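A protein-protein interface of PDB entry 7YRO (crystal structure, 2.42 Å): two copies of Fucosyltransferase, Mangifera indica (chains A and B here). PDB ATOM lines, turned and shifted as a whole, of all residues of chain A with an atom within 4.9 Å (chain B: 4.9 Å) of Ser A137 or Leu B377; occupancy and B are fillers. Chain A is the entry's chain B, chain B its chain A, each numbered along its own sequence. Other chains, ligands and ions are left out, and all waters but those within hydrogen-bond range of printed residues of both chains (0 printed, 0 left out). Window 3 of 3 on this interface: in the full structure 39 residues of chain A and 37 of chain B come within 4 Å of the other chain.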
ATOM      1  N   GLU A 110     -18.928  14.161 -25.623  1.00  0.00           N
ATOM      2  CA  GLU A 110     -17.593  14.309 -25.060  1.00  0.00           C
ATOM      3  C   GLU A 110     -16.515  14.428 -26.131  1.00  0.00           C
ATOM      4  O   GLU A 110     -15.399  14.860 -25.821  1.00  0.00           O
ATOM      5  CB  GLU A 110     -17.297  13.131 -24.132  1.00  0.00           C
ATOM      6  CG  GLU A 110     -17.241  11.788 -24.840  1.00  0.00           C
ATOM      7  CD  GLU A 110     -17.023  10.638 -23.879  1.00  0.00           C
ATOM      8  OE1 GLU A 110     -17.155  10.854 -22.654  1.00  0.00           O
ATOM      9  OE2 GLU A 110     -16.715   9.522 -24.349  1.00  0.00           O
ATOM     10  N   HIS A 111     -16.822  14.057 -27.376  1.00  0.00           N
ATOM     11  CA  HIS A 111     -15.898  14.189 -28.495  1.00  0.00           C
ATOM     12  C   HIS A 111     -16.656  14.681 -29.720  1.00  0.00           C
ATOM     13  O   HIS A 111     -17.748  14.189 -30.019  1.00  0.00           O
ATOM     14  CB  HIS A 111     -15.206  12.860 -28.822  1.00  0.00           C
ATOM     15  CG  HIS A 111     -14.325  12.922 -30.032  1.00  0.00           C
ATOM     16  ND1 HIS A 111     -13.048  13.443 -29.995  1.00  0.00           N
ATOM     17  CD2 HIS A 111     -14.538  12.545 -31.315  1.00  0.00           C
ATOM     18  CE1 HIS A 111     -12.511  13.376 -31.201  1.00  0.00           C
ATOM     19  NE2 HIS A 111     -13.395  12.835 -32.020  1.00  0.00           N
ATOM     20  N   VAL A 112     -16.069  15.644 -30.430  1.00  0.00           N
ATOM     21  CA  VAL A 112     -16.659  16.218 -31.636  1.00  0.00           C
ATOM     22  C   VAL A 112     -15.607  16.239 -32.738  1.00  0.00           C
ATOM     23  O   VAL A 112     -14.443  16.576 -32.492  1.00  0.00           O
ATOM     24  CB  VAL A 112     -17.215  17.639 -31.382  1.00  0.00           C
ATOM     25  CG1 VAL A 112     -17.683  18.285 -32.684  1.00  0.00           C
ATOM     26  CG2 VAL A 112     -18.354  17.598 -30.377  1.00  0.00           C
ATOM     27  N   LEU A 129      -5.963  17.573 -33.064  1.00  0.00           N
ATOM     28  CA  LEU A 129      -6.852  16.953 -32.082  1.00  0.00           C
ATOM     29  C   LEU A 129      -6.721  17.768 -30.797  1.00  0.00           C
ATOM     30  O   LEU A 129      -5.819  17.549 -29.988  1.00  0.00           O
ATOM     31  CB  LEU A 129      -6.501  15.485 -31.886  1.00  0.00           C
ATOM     32  CG  LEU A 129      -7.290  14.697 -30.843  1.00  0.00           C
ATOM     33  CD1 LEU A 129      -8.784  14.792 -31.111  1.00  0.00           C
ATOM     34  CD2 LEU A 129      -6.839  13.246 -30.840  1.00  0.00           C
ATOM     35  N   TYR A 130      -7.603  18.751 -30.640  1.00  0.00           N
ATOM     36  CA  TYR A 130      -7.579  19.665 -29.510  1.00  0.00           C
ATOM     37  C   TYR A 130      -8.231  19.052 -28.278  1.00  0.00           C
ATOM     38  O   TYR A 130      -9.195  18.284 -28.369  1.00  0.00           O
ATOM     39  CB  TYR A 130      -8.313  20.967 -29.850  1.00  0.00           C
ATOM     40  CG  TYR A 130      -7.721  21.779 -30.980  1.00  0.00           C
ATOM     41  CD1 TYR A 130      -8.070  21.526 -32.300  1.00  0.00           C
ATOM     42  CD2 TYR A 130      -6.838  22.815 -30.726  1.00  0.00           C
ATOM     43  CE1 TYR A 130      -7.540  22.270 -33.338  1.00  0.00           C
ATOM     44  CE2 TYR A 130      -6.303  23.566 -31.758  1.00  0.00           C
ATOM     45  CZ  TYR A 130      -6.658  23.289 -33.063  1.00  0.00           C
ATOM     46  OH  TYR A 130      -6.129  24.035 -34.093  1.00  0.00           O
ATOM     47  N   SER A 131      -7.695  19.415 -27.113  1.00  0.00           N
ATOM     48  CA  SER A 131      -8.319  19.162 -25.821  1.00  0.00           C
ATOM     49  C   SER A 131      -8.861  20.486 -25.296  1.00  0.00           C
ATOM     50  O   SER A 131      -8.089  21.421 -25.049  1.00  0.00           O
ATOM     51  CB  SER A 131      -7.324  18.554 -24.833  1.00  0.00           C
ATOM     52  OG  SER A 131      -7.979  18.166 -23.636  1.00  0.00           O
ATOM     53  N   GLY A 135     -13.531  18.761 -20.451  1.00  0.00           N
ATOM     54  CA  GLY A 135     -13.182  17.421 -20.892  1.00  0.00           C
ATOM     55  C   GLY A 135     -13.604  17.071 -22.301  1.00  0.00           C
ATOM     56  O   GLY A 135     -13.819  15.892 -22.602  1.00  0.00           O
ATOM     57  N   LEU A 136     -13.735  18.063 -23.175  1.00  0.00           N
ATOM     58  CA  LEU A 136     -14.160  17.846 -24.552  1.00  0.00           C
ATOM     59  C   LEU A 136     -12.952  17.660 -25.463  1.00  0.00           C
ATOM     60  O   LEU A 136     -11.944  18.355 -25.322  1.00  0.00           O
ATOM     61  CB  LEU A 136     -15.007  19.025 -25.031  1.00  0.00           C
ATOM     62  CG  LEU A 136     -15.378  19.112 -26.512  1.00  0.00           C
ATOM     63  CD1 LEU A 136     -16.415  18.068 -26.873  1.00  0.00           C
ATOM     64  CD2 LEU A 136     -15.880  20.501 -26.845  1.00  0.00           C
ATOM     65  N   SER A 137     -13.021  16.673 -26.352  1.00  0.00           N
ATOM     66  CA  SER A 137     -12.016  16.509 -27.391  1.00  0.00           C
ATOM     67  C   SER A 137     -12.595  16.937 -28.735  1.00  0.00           C
ATOM     68  O   SER A 137     -13.787  16.758 -29.004  1.00  0.00           O
ATOM     69  CB  SER A 137     -11.499  15.065 -27.463  1.00  0.00           C
ATOM     70  OG  SER A 137     -12.553  14.129 -27.594  1.00  0.00           O
ATOM     71  N   CYS A 138     -11.743  17.517 -29.580  1.00  0.00           N
ATOM     72  CA  CYS A 138     -12.189  18.176 -30.805  1.00  0.00           C
ATOM     73  C   CYS A 138     -11.204  17.872 -31.925  1.00  0.00           C
ATOM     74  O   CYS A 138     -10.098  18.413 -31.932  1.00  0.00           O
ATOM     75  CB  CYS A 138     -12.312  19.684 -30.578  1.00  0.00           C
ATOM     76  SG  CYS A 138     -12.735  20.701 -32.020  1.00  0.00           S
ATOM     77  N   LEU A 139     -11.600  17.035 -32.880  1.00  0.00           N
ATOM     78  CA  LEU A 139     -10.727  16.657 -33.990  1.00  0.00           C
ATOM     79  C   LEU A 139     -11.077  17.503 -35.209  1.00  0.00           C
ATOM     80  O   LEU A 139     -12.097  17.266 -35.860  1.00  0.00           O
ATOM     81  CB  LEU A 139     -10.854  15.168 -34.307  1.00  0.00           C
ATOM     82  CG  LEU A 139     -10.033  14.687 -35.511  1.00  0.00           C
ATOM     83  CD1 LEU A 139      -8.600  15.196 -35.432  1.00  0.00           C
ATOM     84  CD2 LEU A 139     -10.060  13.169 -35.618  1.00  0.00           C
ATOM     85  N   VAL B 334      -1.720   6.859 -24.158  1.00  0.00           N
ATOM     86  CA  VAL B 334      -2.276   6.611 -25.485  1.00  0.00           C
ATOM     87  C   VAL B 334      -3.747   6.239 -25.339  1.00  0.00           C
ATOM     88  O   VAL B 334      -4.181   5.848 -24.246  1.00  0.00           O
ATOM     89  CB  VAL B 334      -1.489   5.511 -26.217  1.00  0.00           C
ATOM     90  CG1 VAL B 334      -0.028   5.913 -26.358  1.00  0.00           C
ATOM     91  CG2 VAL B 334      -1.629   4.179 -25.491  1.00  0.00           C
ATOM     92  N   PRO B 335      -4.553   6.374 -26.388  1.00  0.00           N
ATOM     93  CA  PRO B 335      -5.955   5.963 -26.300  1.00  0.00           C
ATOM     94  C   PRO B 335      -6.073   4.451 -26.259  1.00  0.00           C
ATOM     95  O   PRO B 335      -5.120   3.735 -26.606  1.00  0.00           O
ATOM     96  CB  PRO B 335      -6.581   6.552 -27.575  1.00  0.00           C
ATOM     97  CG  PRO B 335      -5.452   6.763 -28.499  1.00  0.00           C
ATOM     98  CD  PRO B 335      -4.242   7.033 -27.669  1.00  0.00           C
ATOM     99  N   PRO B 336      -7.222   3.925 -25.829  1.00  0.00           N
ATOM    100  CA  PRO B 336      -7.384   2.468 -25.754  1.00  0.00           C
ATOM    101  C   PRO B 336      -7.278   1.809 -27.120  1.00  0.00           C
ATOM    102  O   PRO B 336      -7.789   2.319 -28.118  1.00  0.00           O
ATOM    103  CB  PRO B 336      -8.786   2.298 -25.156  1.00  0.00           C
ATOM    104  CG  PRO B 336      -9.489   3.572 -25.471  1.00  0.00           C
ATOM    105  CD  PRO B 336      -8.435   4.633 -25.383  1.00  0.00           C
ATOM    106  N   TRP B 371     -10.721   4.185 -31.663  1.00  0.00           N
ATOM    107  CA  TRP B 371     -10.564   5.214 -30.637  1.00  0.00           C
ATOM    108  C   TRP B 371     -10.807   6.601 -31.219  1.00  0.00           C
ATOM    109  O   TRP B 371     -11.424   7.461 -30.575  1.00  0.00           O
ATOM    110  CB  TRP B 371      -9.173   5.129 -30.005  1.00  0.00           C
ATOM    111  CG  TRP B 371      -8.052   5.486 -30.947  1.00  0.00           C
ATOM    112  CD1 TRP B 371      -7.326   4.624 -31.715  1.00  0.00           C
ATOM    113  CD2 TRP B 371      -7.532   6.794 -31.218  1.00  0.00           C
ATOM    114  NE1 TRP B 371      -6.391   5.310 -32.449  1.00  0.00           N
ATOM    115  CE2 TRP B 371      -6.496   6.646 -32.162  1.00  0.00           C
ATOM    116  CE3 TRP B 371      -7.845   8.077 -30.761  1.00  0.00           C
ATOM    117  CZ2 TRP B 371      -5.772   7.729 -32.653  1.00  0.00           C
ATOM    118  CZ3 TRP B 371      -7.124   9.149 -31.247  1.00  0.00           C
ATOM    119  CH2 TRP B 371      -6.100   8.969 -32.183  1.00  0.00           C
ATOM    120  N   GLY B 375     -14.559   8.441 -30.802  1.00  0.00           N
ATOM    121  CA  GLY B 375     -14.326   9.423 -29.761  1.00  0.00           C
ATOM    122  C   GLY B 375     -14.104   8.835 -28.384  1.00  0.00           C
ATOM    123  O   GLY B 375     -14.588   9.392 -27.389  1.00  0.00           O
ATOM    124  N   VAL B 376     -13.393   7.711 -28.299  1.00  0.00           N
ATOM    125  CA  VAL B 376     -13.018   7.149 -27.007  1.00  0.00           C
ATOM    126  C   VAL B 376     -11.514   7.310 -26.864  1.00  0.00           C
ATOM    127  O   VAL B 376     -10.740   6.429 -27.254  1.00  0.00           O
ATOM    128  CB  VAL B 376     -13.441   5.675 -26.878  1.00  0.00           C
ATOM    129  CG1 VAL B 376     -13.202   5.187 -25.457  1.00  0.00           C
ATOM    130  CG2 VAL B 376     -14.901   5.504 -27.275  1.00  0.00           C
ATOM    131  N   LEU B 377     -11.096   8.440 -26.296  1.00  0.00           N
ATOM    132  CA  LEU B 377      -9.687   8.795 -26.217  1.00  0.00           C
ATOM    133  C   LEU B 377      -8.992   8.220 -24.993  1.00  0.00           C
ATOM    134  O   LEU B 377      -7.757   8.153 -24.974  1.00  0.00           O
ATOM    135  CB  LEU B 377      -9.525  10.319 -26.216  1.00  0.00           C
ATOM    136  CG  LEU B 377      -9.883  11.060 -27.509  1.00  0.00           C
ATOM    137  CD1 LEU B 377      -9.115  12.374 -27.609  1.00  0.00           C
ATOM    138  CD2 LEU B 377      -9.643  10.193 -28.730  1.00  0.00           C
ATOM    139  N   GLY B 378      -9.745   7.825 -23.976  1.00  0.00           N
ATOM    140  CA  GLY B 378      -9.114   7.324 -22.770  1.00  0.00           C
ATOM    141  C   GLY B 378      -8.244   8.400 -22.163  1.00  0.00           C
ATOM    142  O   GLY B 378      -8.702   9.507 -21.856  1.00  0.00           O
ATOM    143  N   ASN B 379      -6.963   8.084 -21.999  1.00  0.00           N
ATOM    144  CA  ASN B 379      -6.011   9.010 -21.407  1.00  0.00           C
ATOM    145  C   ASN B 379      -5.363   9.940 -22.425  1.00  0.00           C
ATOM    146  O   ASN B 379      -4.666  10.879 -22.025  1.00  0.00           O
ATOM    147  CB  ASN B 379      -4.922   8.218 -20.679  1.00  0.00           C
ATOM    148  CG  ASN B 379      -5.486   7.299 -19.613  1.00  0.00           C
ATOM    149  OD1 ASN B 379      -6.329   7.701 -18.811  1.00  0.00           O
ATOM    150  ND2 ASN B 379      -5.026   6.051 -19.607  1.00  0.00           N
ATOM    151  N   TYR B 380      -5.576   9.701 -23.722  1.00  0.00           N
ATOM    152  CA  TYR B 380      -4.941  10.516 -24.753  1.00  0.00           C
ATOM    153  C   TYR B 380      -5.364  11.974 -24.669  1.00  0.00           C
ATOM    154  O   TYR B 380      -4.561  12.873 -24.959  1.00  0.00           O
ATOM    155  CB  TYR B 380      -5.266   9.942 -26.130  1.00  0.00           C
ATOM    156  CG  TYR B 380      -4.406  10.473 -27.253  1.00  0.00           C
ATOM    157  CD1 TYR B 380      -3.099  10.872 -27.024  1.00  0.00           C
ATOM    158  CD2 TYR B 380      -4.893  10.537 -28.552  1.00  0.00           C
ATOM    159  CE1 TYR B 380      -2.307  11.348 -28.056  1.00  0.00           C
ATOM    160  CE2 TYR B 380      -4.109  11.007 -29.590  1.00  0.00           C
ATOM    161  CZ  TYR B 380      -2.817  11.413 -29.338  1.00  0.00           C
ATOM    162  OH  TYR B 380      -2.036  11.880 -30.370  1.00  0.00           O
ATOM    163  N   GLY B 381      -6.614  12.234 -24.287  1.00  0.00           N
ATOM    164  CA  GLY B 381      -7.051  13.612 -24.140  1.00  0.00           C
ATOM    165  C   GLY B 381      -6.234  14.356 -23.104  1.00  0.00           C
ATOM    166  O   GLY B 381      -5.763  15.475 -23.344  1.00  0.00           O
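Of the printed residues of chain B, Glu A110 touches Gly B375 (3.7 Å).
Of the printed residues of chain B, His A111 touches Gly B375.
Printed residues of chain B within 4 Å of Leu A129: Tyr B380 (3.7 Å).
Leu A136 touches none of the printed residues of chain B.
Ser A137 touches just one residue of chain B: Leu B377 (3.6 Å).
Of the printed residues of chain A, Gly B375 touches Glu A110 and His A111.
Val B376 touches none of the printed residues of chain A.
Of chain A, only Ser A137 (3.6 Å) comes within 4 Å of Leu B377.
Of the printed residues of chain A, Tyr B380 touches Leu A129.
The nearest printed residue of chain B that does not touch Ser A137 is Gly B375 (5.2 Å).
No position is printed for both chains.
Of the 5 pairs that touch across the chains among the printed residues, none has its exchanged pair printed and touching as well.
Among the printed residues, pairs that only touch across the chains: His A111 with Gly B375 (3.5 Å), Ser A137 with Leu B377 (3.6 Å), Glu A110 with Gly B375 (3.7 Å) and Leu A129 with Tyr B380 (3.7 Å).
The side-chain hydroxyl (OG) of Ser A131 sits at hydrogen-bond distance from the backbone carbonyl oxygen (O) of Gly B381 (3.5 Å).
Of the 11 printed residues of chain A, 5 touch a printed residue of chain B.
Along chain A the printed residues that touch a printed residue of chain B span positions 110 to 137.
Among the printed residues, 5 pairs touch across the chains.
Among the printed residues, no Asp or Glu carboxylate lies within 4 Å of a Lys or Arg side-chain nitrogen of the other chain.
O of Ser A137 is in hydrogen-bond range of N of Val A112.
ND1 of His A111 lies within hydrogen-bond range of OG of Ser A137, at 2.5 Å.
The backbone NH (N) of Ser A137 sits at hydrogen-bond distance from the backbone carbonyl oxygen (O) of Glu A110 (3.0 Å).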
